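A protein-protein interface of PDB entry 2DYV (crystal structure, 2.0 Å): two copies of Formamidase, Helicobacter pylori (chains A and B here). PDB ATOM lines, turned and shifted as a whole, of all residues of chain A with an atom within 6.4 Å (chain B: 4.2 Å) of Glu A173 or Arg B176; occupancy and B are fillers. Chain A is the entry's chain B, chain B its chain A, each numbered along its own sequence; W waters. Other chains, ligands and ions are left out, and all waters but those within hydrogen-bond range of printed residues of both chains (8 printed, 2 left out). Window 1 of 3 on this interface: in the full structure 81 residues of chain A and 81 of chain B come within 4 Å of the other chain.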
ATOM      1  N   MET A 170      27.454 -28.799 -13.209  1.00  0.00           N
ATOM      2  CA  MET A 170      27.076 -27.396 -13.364  1.00  0.00           C
ATOM      3  C   MET A 170      26.007 -26.936 -12.371  1.00  0.00           C
ATOM      4  O   MET A 170      25.723 -25.749 -12.280  1.00  0.00           O
ATOM      5  CB  MET A 170      26.609 -27.104 -14.796  1.00  0.00           C
ATOM      6  CG  MET A 170      27.672 -27.307 -15.895  1.00  0.00           C
ATOM      7  SD  MET A 170      29.266 -26.517 -15.530  1.00  0.00           S
ATOM      8  CE  MET A 170      28.782 -25.380 -14.245  1.00  0.00           C
ATOM      9  N   ILE A 171      25.430 -27.883 -11.636  1.00  0.00           N
ATOM     10  CA  ILE A 171      24.339 -27.613 -10.710  1.00  0.00           C
ATOM     11  C   ILE A 171      24.867 -27.653  -9.274  1.00  0.00           C
ATOM     12  O   ILE A 171      25.148 -28.726  -8.766  1.00  0.00           O
ATOM     13  CB  ILE A 171      23.195 -28.646 -10.856  1.00  0.00           C
ATOM     14  CG1 ILE A 171      22.813 -28.862 -12.338  1.00  0.00           C
ATOM     15  CG2 ILE A 171      21.975 -28.231  -9.972  1.00  0.00           C
ATOM     16  CD1 ILE A 171      22.079 -27.672 -13.016  1.00  0.00           C
ATOM     17  N   PRO A 172      25.028 -26.477  -8.630  1.00  0.00           N
ATOM     18  CA  PRO A 172      25.579 -26.433  -7.263  1.00  0.00           C
ATOM     19  C   PRO A 172      24.714 -27.133  -6.210  1.00  0.00           C
ATOM     20  O   PRO A 172      25.241 -27.632  -5.220  1.00  0.00           O
ATOM     21  CB  PRO A 172      25.664 -24.935  -6.963  1.00  0.00           C
ATOM     22  CG  PRO A 172      24.666 -24.300  -7.886  1.00  0.00           C
ATOM     23  CD  PRO A 172      24.725 -25.129  -9.141  1.00  0.00           C
ATOM     24  N   GLU A 173      23.401 -27.142  -6.415  1.00  0.00           N
ATOM     25  CA  GLU A 173      22.489 -27.803  -5.486  1.00  0.00           C
ATOM     26  C   GLU A 173      22.742 -29.299  -5.426  1.00  0.00           C
ATOM     27  O   GLU A 173      22.475 -29.931  -4.412  1.00  0.00           O
ATOM     28  CB  GLU A 173      21.033 -27.539  -5.873  1.00  0.00           C
ATOM     29  CG  GLU A 173      20.592 -26.081  -5.666  1.00  0.00           C
ATOM     30  CD  GLU A 173      20.828 -25.192  -6.871  1.00  0.00           C
ATOM     31  OE1 GLU A 173      21.431 -25.670  -7.870  1.00  0.00           O
ATOM     32  OE2 GLU A 173      20.404 -24.003  -6.818  1.00  0.00           O
ATOM     33  N   LEU A 174      23.249 -29.863  -6.524  1.00  0.00           N
ATOM     34  CA  LEU A 174      23.584 -31.291  -6.562  1.00  0.00           C
ATOM     35  C   LEU A 174      24.842 -31.620  -5.772  1.00  0.00           C
ATOM     36  O   LEU A 174      24.883 -32.638  -5.063  1.00  0.00           O
ATOM     37  CB  LEU A 174      23.719 -31.785  -8.000  1.00  0.00           C
ATOM     38  CG  LEU A 174      23.747 -33.298  -8.175  1.00  0.00           C
ATOM     39  CD1 LEU A 174      22.649 -33.978  -7.335  1.00  0.00           C
ATOM     40  CD2 LEU A 174      23.616 -33.653  -9.653  1.00  0.00           C
ATOM     41  N   ALA A 175      25.872 -30.770  -5.894  1.00  0.00           N
ATOM     42  CA  ALA A 175      27.042 -30.910  -5.045  1.00  0.00           C
ATOM     43  C   ALA A 175      26.659 -30.763  -3.567  1.00  0.00           C
ATOM     44  O   ALA A 175      27.139 -31.514  -2.714  1.00  0.00           O
ATOM     45  CB  ALA A 175      28.114 -29.901  -5.424  1.00  0.00           C
ATOM     46  N   ARG A 176      25.793 -29.799  -3.274  1.00  0.00           N
ATOM     47  CA  ARG A 176      25.296 -29.600  -1.904  1.00  0.00           C
ATOM     48  C   ARG A 176      24.593 -30.863  -1.380  1.00  0.00           C
ATOM     49  O   ARG A 176      24.832 -31.277  -0.258  1.00  0.00           O
ATOM     50  CB  ARG A 176      24.374 -28.367  -1.835  1.00  0.00           C
ATOM     51  CG  ARG A 176      23.826 -28.007  -0.433  1.00  0.00           C
ATOM     52  CD  ARG A 176      24.848 -27.350   0.467  1.00  0.00           C
ATOM     53  NE  ARG A 176      24.995 -25.934   0.143  1.00  0.00           N
ATOM     54  CZ  ARG A 176      26.066 -25.200   0.414  1.00  0.00           C
ATOM     55  NH1 ARG A 176      27.132 -25.740   0.991  1.00  0.00           N
ATOM     56  NH2 ARG A 176      26.068 -23.916   0.096  1.00  0.00           N
ATOM     57  N   GLU A 177      23.747 -31.469  -2.209  1.00  0.00           N
ATOM     58  CA  GLU A 177      23.053 -32.695  -1.847  1.00  0.00           C
ATOM     59  C   GLU A 177      24.023 -33.831  -1.500  1.00  0.00           C
ATOM     60  O   GLU A 177      23.836 -34.504  -0.486  1.00  0.00           O
ATOM     61  CB  GLU A 177      22.075 -33.127  -2.949  1.00  0.00           C
ATOM     62  CG  GLU A 177      21.290 -34.420  -2.667  1.00  0.00           C
ATOM     63  CD  GLU A 177      20.289 -34.309  -1.521  1.00  0.00           C
ATOM     64  OE1 GLU A 177      20.089 -33.209  -0.963  1.00  0.00           O
ATOM     65  OE2 GLU A 177      19.693 -35.348  -1.160  1.00  0.00           O
ATOM     66  N   ALA A 178      25.064 -34.019  -2.316  1.00  0.00           N
ATOM     67  CA  ALA A 178      26.063 -35.039  -2.020  1.00  0.00           C
ATOM     68  C   ALA A 178      26.676 -34.796  -0.640  1.00  0.00           C
ATOM     69  O   ALA A 178      26.719 -35.709   0.188  1.00  0.00           O
ATOM     70  CB  ALA A 178      27.146 -35.091  -3.102  1.00  0.00           C
ATOM     71  N   ASN A 207      32.350 -26.390  -6.442  1.00  0.00           N
ATOM     72  CA  ASN A 207      31.677 -27.547  -5.823  1.00  0.00           C
ATOM     73  C   ASN A 207      32.423 -28.028  -4.585  1.00  0.00           C
ATOM     74  O   ASN A 207      31.811 -28.420  -3.589  1.00  0.00           O
ATOM     75  CB  ASN A 207      31.542 -28.693  -6.830  1.00  0.00           C
ATOM     76  CG  ASN A 207      30.394 -28.489  -7.802  1.00  0.00           C
ATOM     77  OD1 ASN A 207      29.526 -27.632  -7.591  1.00  0.00           O
ATOM     78  ND2 ASN A 207      30.366 -29.291  -8.868  1.00  0.00           N
ATOM     79  N   TYR A 298      12.903 -19.722  -3.990  1.00  0.00           N
ATOM     80  CA  TYR A 298      13.156 -20.804  -4.947  1.00  0.00           C
ATOM     81  C   TYR A 298      13.227 -22.157  -4.252  1.00  0.00           C
ATOM     82  O   TYR A 298      12.776 -23.168  -4.801  1.00  0.00           O
ATOM     83  CB  TYR A 298      14.389 -20.529  -5.831  1.00  0.00           C
ATOM     84  CG  TYR A 298      15.713 -21.192  -5.457  1.00  0.00           C
ATOM     85  CD1 TYR A 298      16.024 -22.471  -5.907  1.00  0.00           C
ATOM     86  CD2 TYR A 298      16.677 -20.511  -4.714  1.00  0.00           C
ATOM     87  CE1 TYR A 298      17.230 -23.068  -5.605  1.00  0.00           C
ATOM     88  CE2 TYR A 298      17.888 -21.105  -4.401  1.00  0.00           C
ATOM     89  CZ  TYR A 298      18.162 -22.383  -4.856  1.00  0.00           C
ATOM     90  OH  TYR A 298      19.366 -22.982  -4.587  1.00  0.00           O
ATOM     91  N   ILE A 299      13.775 -22.162  -3.037  1.00  0.00           N
ATOM     92  CA  ILE A 299      13.906 -23.385  -2.256  1.00  0.00           C
ATOM     93  C   ILE A 299      12.533 -23.959  -1.905  1.00  0.00           C
ATOM     94  O   ILE A 299      12.295 -25.163  -2.030  1.00  0.00           O
ATOM     95  CB  ILE A 299      14.705 -23.129  -0.955  1.00  0.00           C
ATOM     96  CG1 ILE A 299      16.143 -22.674  -1.268  1.00  0.00           C
ATOM     97  CG2 ILE A 299      14.657 -24.329  -0.063  1.00  0.00           C
ATOM     98  CD1 ILE A 299      17.056 -23.745  -1.768  1.00  0.00           C
ATOM     99  N   LEU A 302      10.824 -25.159  -5.332  1.00  0.00           N
ATOM    100  CA  LEU A 302      11.378 -26.429  -5.812  1.00  0.00           C
ATOM    101  C   LEU A 302      11.010 -27.626  -4.926  1.00  0.00           C
ATOM    102  O   LEU A 302      10.800 -28.731  -5.433  1.00  0.00           O
ATOM    103  CB  LEU A 302      12.897 -26.313  -5.987  1.00  0.00           C
ATOM    104  CG  LEU A 302      13.704 -27.314  -6.809  1.00  0.00           C
ATOM    105  CD1 LEU A 302      13.288 -27.357  -8.274  1.00  0.00           C
ATOM    106  CD2 LEU A 302      15.174 -26.948  -6.710  1.00  0.00           C
ATOM    107  N   TYR A 307       8.961 -24.754  -9.087  1.00  0.00           N
ATOM    108  CA  TYR A 307      10.041 -23.893  -9.564  1.00  0.00           C
ATOM    109  C   TYR A 307       9.638 -23.313 -10.903  1.00  0.00           C
ATOM    110  O   TYR A 307       9.399 -24.050 -11.869  1.00  0.00           O
ATOM    111  CB  TYR A 307      11.309 -24.721  -9.724  1.00  0.00           C
ATOM    112  CG  TYR A 307      12.576 -23.983 -10.122  1.00  0.00           C
ATOM    113  CD1 TYR A 307      13.491 -23.564  -9.154  1.00  0.00           C
ATOM    114  CD2 TYR A 307      12.902 -23.773 -11.464  1.00  0.00           C
ATOM    115  CE1 TYR A 307      14.673 -22.920  -9.504  1.00  0.00           C
ATOM    116  CE2 TYR A 307      14.093 -23.129 -11.831  1.00  0.00           C
ATOM    117  CZ  TYR A 307      14.972 -22.714 -10.837  1.00  0.00           C
ATOM    118  OH  TYR A 307      16.149 -22.091 -11.169  1.00  0.00           O
ATOM    119  N   PRO B 172      25.869 -20.356  -2.635  1.00  0.00           N
ATOM    120  CA  PRO B 172      25.393 -20.393  -4.022  1.00  0.00           C
ATOM    121  C   PRO B 172      23.871 -20.345  -4.138  1.00  0.00           C
ATOM    122  O   PRO B 172      23.350 -19.881  -5.166  1.00  0.00           O
ATOM    123  CB  PRO B 172      25.926 -21.737  -4.553  1.00  0.00           C
ATOM    124  CG  PRO B 172      26.127 -22.574  -3.360  1.00  0.00           C
ATOM    125  CD  PRO B 172      26.587 -21.596  -2.287  1.00  0.00           C
ATOM    126  N   GLU B 173      23.167 -20.819  -3.104  1.00  0.00           N
ATOM    127  CA  GLU B 173      21.701 -20.790  -3.088  1.00  0.00           C
ATOM    128  C   GLU B 173      21.165 -19.363  -3.095  1.00  0.00           C
ATOM    129  O   GLU B 173      20.090 -19.110  -3.619  1.00  0.00           O
ATOM    130  CB  GLU B 173      21.146 -21.554  -1.874  1.00  0.00           C
ATOM    131  CG  GLU B 173      21.330 -23.066  -1.944  1.00  0.00           C
ATOM    132  CD  GLU B 173      22.678 -23.562  -1.460  1.00  0.00           C
ATOM    133  OE1 GLU B 173      23.569 -22.732  -1.158  1.00  0.00           O
ATOM    134  OE2 GLU B 173      22.851 -24.808  -1.399  1.00  0.00           O
ATOM    135  N   LEU B 174      21.925 -18.435  -2.514  1.00  0.00           N
ATOM    136  CA  LEU B 174      21.507 -17.043  -2.442  1.00  0.00           C
ATOM    137  C   LEU B 174      21.644 -16.333  -3.792  1.00  0.00           C
ATOM    138  O   LEU B 174      20.817 -15.502  -4.133  1.00  0.00           O
ATOM    139  CB  LEU B 174      22.297 -16.297  -1.362  1.00  0.00           C
ATOM    140  CG  LEU B 174      21.854 -14.862  -1.081  1.00  0.00           C
ATOM    141  CD1 LEU B 174      20.355 -14.823  -0.766  1.00  0.00           C
ATOM    142  CD2 LEU B 174      22.690 -14.232   0.055  1.00  0.00           C
ATOM    143  N   ALA B 175      22.694 -16.641  -4.547  1.00  0.00           N
ATOM    144  CA  ALA B 175      22.827 -16.104  -5.906  1.00  0.00           C
ATOM    145  C   ALA B 175      21.706 -16.643  -6.785  1.00  0.00           C
ATOM    146  O   ALA B 175      21.121 -15.904  -7.601  1.00  0.00           O
ATOM    147  CB  ALA B 175      24.190 -16.429  -6.499  1.00  0.00           C
ATOM    148  N   ARG B 176      21.387 -17.923  -6.594  1.00  0.00           N
ATOM    149  CA  ARG B 176      20.243 -18.544  -7.281  1.00  0.00           C
ATOM    150  C   ARG B 176      18.931 -17.813  -6.984  1.00  0.00           C
ATOM    151  O   ARG B 176      18.142 -17.541  -7.884  1.00  0.00           O
ATOM    152  CB  ARG B 176      20.110 -20.022  -6.898  1.00  0.00           C
ATOM    153  CG  ARG B 176      18.997 -20.763  -7.644  1.00  0.00           C
ATOM    154  CD  ARG B 176      19.413 -21.036  -9.077  1.00  0.00           C
ATOM    155  NE  ARG B 176      20.242 -22.227  -9.159  1.00  0.00           N
ATOM    156  CZ  ARG B 176      21.017 -22.534 -10.196  1.00  0.00           C
ATOM    157  NH1 ARG B 176      21.103 -21.713 -11.237  1.00  0.00           N
ATOM    158  NH2 ARG B 176      21.711 -23.665 -10.184  1.00  0.00           N
ATOM    159  N   GLU B 177      18.694 -17.525  -5.710  1.00  0.00           N
ATOM    160  CA  GLU B 177      17.497 -16.811  -5.294  1.00  0.00           C
ATOM    161  C   GLU B 177      17.381 -15.460  -5.978  1.00  0.00           C
ATOM    162  O   GLU B 177      16.305 -15.118  -6.483  1.00  0.00           O
ATOM    163  CB  GLU B 177      17.475 -16.620  -3.774  1.00  0.00           C
ATOM    164  CG  GLU B 177      16.308 -15.783  -3.243  1.00  0.00           C
ATOM    165  CD  GLU B 177      14.948 -16.450  -3.396  1.00  0.00           C
ATOM    166  OE1 GLU B 177      14.863 -17.623  -3.818  1.00  0.00           O
ATOM    167  OE2 GLU B 177      13.945 -15.781  -3.091  1.00  0.00           O
ATOM    168  N   ALA B 178      18.476 -14.696  -5.994  1.00  0.00           N
ATOM    169  CA  ALA B 178      18.479 -13.395  -6.669  1.00  0.00           C
ATOM    170  C   ALA B 178      18.077 -13.555  -8.132  1.00  0.00           C
ATOM    171  O   ALA B 178      17.176 -12.856  -8.609  1.00  0.00           O
ATOM    172  CB  ALA B 178      19.850 -12.715  -6.551  1.00  0.00           C
ATOM    173  N   ALA B 179      18.712 -14.512  -8.815  1.00  0.00           N
ATOM    174  CA  ALA B 179      18.412 -14.835 -10.211  1.00  0.00           C
ATOM    175  C   ALA B 179      16.944 -15.238 -10.422  1.00  0.00           C
ATOM    176  O   ALA B 179      16.282 -14.756 -11.351  1.00  0.00           O
ATOM    177  CB  ALA B 179      19.360 -15.946 -10.710  1.00  0.00           C
ATOM    178  N   TYR B 180      16.444 -16.108  -9.542  1.00  0.00           N
ATOM    179  CA  TYR B 180      15.071 -16.628  -9.599  1.00  0.00           C
ATOM    180  C   TYR B 180      14.048 -15.498  -9.516  1.00  0.00           C
ATOM    181  O   TYR B 180      12.949 -15.609 -10.047  1.00  0.00           O
ATOM    182  CB  TYR B 180      14.847 -17.627  -8.452  1.00  0.00           C
ATOM    183  CG  TYR B 180      13.543 -18.418  -8.477  1.00  0.00           C
ATOM    184  CD1 TYR B 180      13.364 -19.485  -9.350  1.00  0.00           C
ATOM    185  CD2 TYR B 180      12.513 -18.133  -7.568  1.00  0.00           C
ATOM    186  CE1 TYR B 180      12.166 -20.232  -9.353  1.00  0.00           C
ATOM    187  CE2 TYR B 180      11.328 -18.861  -7.562  1.00  0.00           C
ATOM    188  CZ  TYR B 180      11.164 -19.914  -8.456  1.00  0.00           C
ATOM    189  OH  TYR B 180       9.999 -20.646  -8.449  1.00  0.00           O
ATOM    190  N   HIS B 210      26.711 -19.812 -12.799  1.00  0.00           N
ATOM    191  CA  HIS B 210      25.602 -20.693 -12.366  1.00  0.00           C
ATOM    192  C   HIS B 210      24.257 -20.148 -12.812  1.00  0.00           C
ATOM    193  O   HIS B 210      23.328 -20.905 -13.108  1.00  0.00           O
ATOM    194  CB  HIS B 210      25.538 -20.812 -10.838  1.00  0.00           C
ATOM    195  CG  HIS B 210      26.538 -21.751 -10.234  1.00  0.00           C
ATOM    196  ND1 HIS B 210      26.937 -22.923 -10.837  1.00  0.00           N
ATOM    197  CD2 HIS B 210      27.172 -21.712  -9.039  1.00  0.00           C
ATOM    198  CE1 HIS B 210      27.800 -23.548 -10.055  1.00  0.00           C
ATOM    199  NE2 HIS B 210      27.954 -22.833  -8.955  1.00  0.00           N
ATOM    200  N   ASN B 211      24.160 -18.822 -12.834  1.00  0.00           N
ATOM    201  CA  ASN B 211      22.875 -18.151 -12.935  1.00  0.00           C
ATOM    202  C   ASN B 211      22.671 -17.304 -14.182  1.00  0.00           C
ATOM    203  O   ASN B 211      21.643 -16.639 -14.318  1.00  0.00           O
ATOM    204  CB  ASN B 211      22.672 -17.307 -11.685  1.00  0.00           C
ATOM    205  CG  ASN B 211      22.572 -18.162 -10.434  1.00  0.00           C
ATOM    206  OD1 ASN B 211      21.584 -18.860 -10.240  1.00  0.00           O
ATOM    207  ND2 ASN B 211      23.610 -18.131  -9.595  1.00  0.00           N
ATOM    208  N   ILE B 276      20.149 -22.820 -15.000  1.00  0.00           N
ATOM    209  CA  ILE B 276      19.113 -22.270 -14.135  1.00  0.00           C
ATOM    210  C   ILE B 276      17.718 -22.791 -14.526  1.00  0.00           C
ATOM    211  O   ILE B 276      16.890 -23.071 -13.652  1.00  0.00           O
ATOM    212  CB  ILE B 276      19.178 -20.717 -14.023  1.00  0.00           C
ATOM    213  CG1 ILE B 276      18.155 -20.210 -12.993  1.00  0.00           C
ATOM    214  CG2 ILE B 276      19.054 -20.023 -15.408  1.00  0.00           C
ATOM    215  CD1 ILE B 276      18.293 -18.763 -12.628  1.00  0.00           C
ATOM    216  N   LEU B 279      17.498 -26.825 -13.650  1.00  0.00           N
ATOM    217  CA  LEU B 279      17.268 -27.139 -12.233  1.00  0.00           C
ATOM    218  C   LEU B 279      15.831 -27.589 -11.924  1.00  0.00           C
ATOM    219  O   LEU B 279      15.627 -28.536 -11.161  1.00  0.00           O
ATOM    220  CB  LEU B 279      17.653 -25.948 -11.336  1.00  0.00           C
ATOM    221  CG  LEU B 279      17.533 -26.139  -9.809  1.00  0.00           C
ATOM    222  CD1 LEU B 279      18.318 -27.371  -9.304  1.00  0.00           C
ATOM    223  CD2 LEU B 279      17.949 -24.882  -9.038  1.00  0.00           C
ATOM    224  N   TYR B 298      18.032 -32.118   0.761  1.00  0.00           N
ATOM    225  CA  TYR B 298      18.369 -30.916   1.528  1.00  0.00           C
ATOM    226  C   TYR B 298      17.446 -29.764   1.194  1.00  0.00           C
ATOM    227  O   TYR B 298      17.116 -28.952   2.063  1.00  0.00           O
ATOM    228  CB  TYR B 298      19.842 -30.524   1.360  1.00  0.00           C
ATOM    229  CG  TYR B 298      20.142 -29.459   0.327  1.00  0.00           C
ATOM    230  CD1 TYR B 298      20.069 -28.096   0.652  1.00  0.00           C
ATOM    231  CD2 TYR B 298      20.561 -29.807  -0.955  1.00  0.00           C
ATOM    232  CE1 TYR B 298      20.377 -27.115  -0.283  1.00  0.00           C
ATOM    233  CE2 TYR B 298      20.860 -28.823  -1.909  1.00  0.00           C
ATOM    234  CZ  TYR B 298      20.775 -27.490  -1.566  1.00  0.00           C
ATOM    235  OH  TYR B 298      21.085 -26.532  -2.499  1.00  0.00           O
HETATM  236  O   HOH W   1      22.672 -22.887  -5.568  1.00  0.00           O
HETATM  237  O   HOH W   2      11.837 -22.666  -7.115  1.00  0.00           O
HETATM  238  O   HOH W   3      23.993 -25.049  -4.318  1.00  0.00           O
HETATM  239  O   HOH W   4      25.741 -25.607  -2.532  1.00  0.00           O
HETATM  240  O   HOH W   5      29.416 -24.875  -7.027  1.00  0.00           O
HETATM  241  O   HOH W   6      23.666 -23.782 -12.216  1.00  0.00           O
HETATM  242  O   HOH W   7      22.685 -21.736  -7.868  1.00  0.00           O
HETATM  243  O   HOH W   8      19.359 -24.938  -3.171  1.00  0.00           O
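OE2 of Glu A173 lies within salt-bridge range of NE of Arg B176. The side-chain carboxylate (OE1) of Glu A177 lies within hydrogen-bond range of the backbone NH (N) of Tyr B298 (2.9 Å). NE of Arg A176 lies within salt-bridge range of OE2 of Glu B173 (2.9 Å). The backbone NH (N) of Tyr A298 is in hydrogen-bond range of the side-chain carboxylate (OE1) of Glu B177 (2.9 Å). The backbone carbonyl oxygen of Met A170 is in hydrogen-bond range of a ring nitrogen (ND1) of His B210. O of Ile B276 lies within hydrogen-bond range of OH of Tyr A307 (2.8 Å).
OH of Tyr B298 is in hydrogen-bond range of OE2 of Glu B173, at 2.7 Å. The guanidinium group (NH1) of Arg B176 lies within hydrogen-bond range of the backbone carbonyl oxygen (O) of His B210. OH of Tyr A298 is in hydrogen-bond range of OE2 of Glu A173 (2.7 Å). The guanidinium group (NH1) of Arg B176 sits at hydrogen-bond distance from the side-chain amide oxygen (OD1) of Asn B211, 3.1 Å away.
Pro A172 touches His B210. CE2 of Tyr B298 touches O of Glu A173, 3.2 Å away. Arg A176 touches Pro B172 (NH2 to CD, 3.4 Å). Tyr B298 touches Arg A176 (CZ to CG, 3.3 Å). Tyr A298 touches Glu B173 (CE2 to O, 3.1 Å). CZ of Tyr A298 touches CG of Arg B176, at 3.3 Å. Tyr A298 touches Leu B279. Leu A302 touches Leu B279. Tyr A307 touches Tyr B180 (CA to OH, 3.4 Å). Tyr A307 touches Leu B279.
Ala A175 touches none of the printed residues of chain B. Of the printed residues of chain A, Arg B176 touches Pro A172, Glu A173 and Tyr A298. Of the printed residues of chain A, Glu B177 touches Tyr A298 (2.9 Å). Of the printed residues of chain A, Tyr B180 touches Tyr A298 (3.5 Å) and Tyr A307 (3.4 Å). The nearest printed residue of chain A that does not touch Tyr B298 is Tyr A298 (4.5 Å).
Hydrophobic or aromatic side chains of chain B within 4 Å of the printed part of chain A: Pro B172, Tyr B180, His B210, Ile B276, Leu B279 and Tyr B298. Along chain A the printed residues that touch a printed residue of chain B span positions 170 to 307. Among the printed residues, 20 pairs touch across the chains. Among the printed residues, Asp or Glu carboxylates within 4 Å of a Lys or Arg side-chain nitrogen of the other chain: Glu A173 with Arg B176 and Arg A176 with Glu B173.
Glu A173 touches Arg B176, and with the chains exchanged Arg A176 touches Glu B173. Glu A173 touches Tyr B298, and with the chains exchanged Tyr A298 touches Glu B173. Arg A176 touches Tyr B298, and with the chains exchanged Tyr A298 touches Arg B176. Glu A177 touches Tyr B298, and with the chains exchanged Tyr A298 touches Glu B177. Of the 20 pairs that touch across the chains among the printed residues, 10 have their exchanged pair printed and touching as well.
Water W2 lies within hydrogen-bond range of O of Tyr A298 (2.5 Å), OH of Tyr B180 (3.0 Å) and N of Leu A302 (3.2 Å). Water W4 lies within hydrogen-bond range of NE of Arg A176 (2.8 Å), OE2 of Glu B173 (3.2 Å) and O of Pro A172 (3.4 Å). Water W7 lies within hydrogen-bond range of NE of Arg B176 (2.8 Å), O of Pro B172 (3.3 Å) and OE2 of Glu A173 (3.4 Å). Water W5 bridges OD1 of Asn A207 (2.8 Å) and NE2 of His B210 (3.2 Å). Water W1 lies within hydrogen-bond range of the side-chain carboxylate of Glu A173 (2.8 Å), the backbone carbonyl oxygen of Pro B172 (3.1 Å), the backbone NH of Glu B173 (3.3 Å) and the side-chain hydroxyl of Tyr A298 (3.4 Å). Water W3 lies within hydrogen-bond range of the backbone carbonyl oxygen of Pro A172, the backbone NH of Glu A173 and the side-chain carboxylate of Glu B173.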
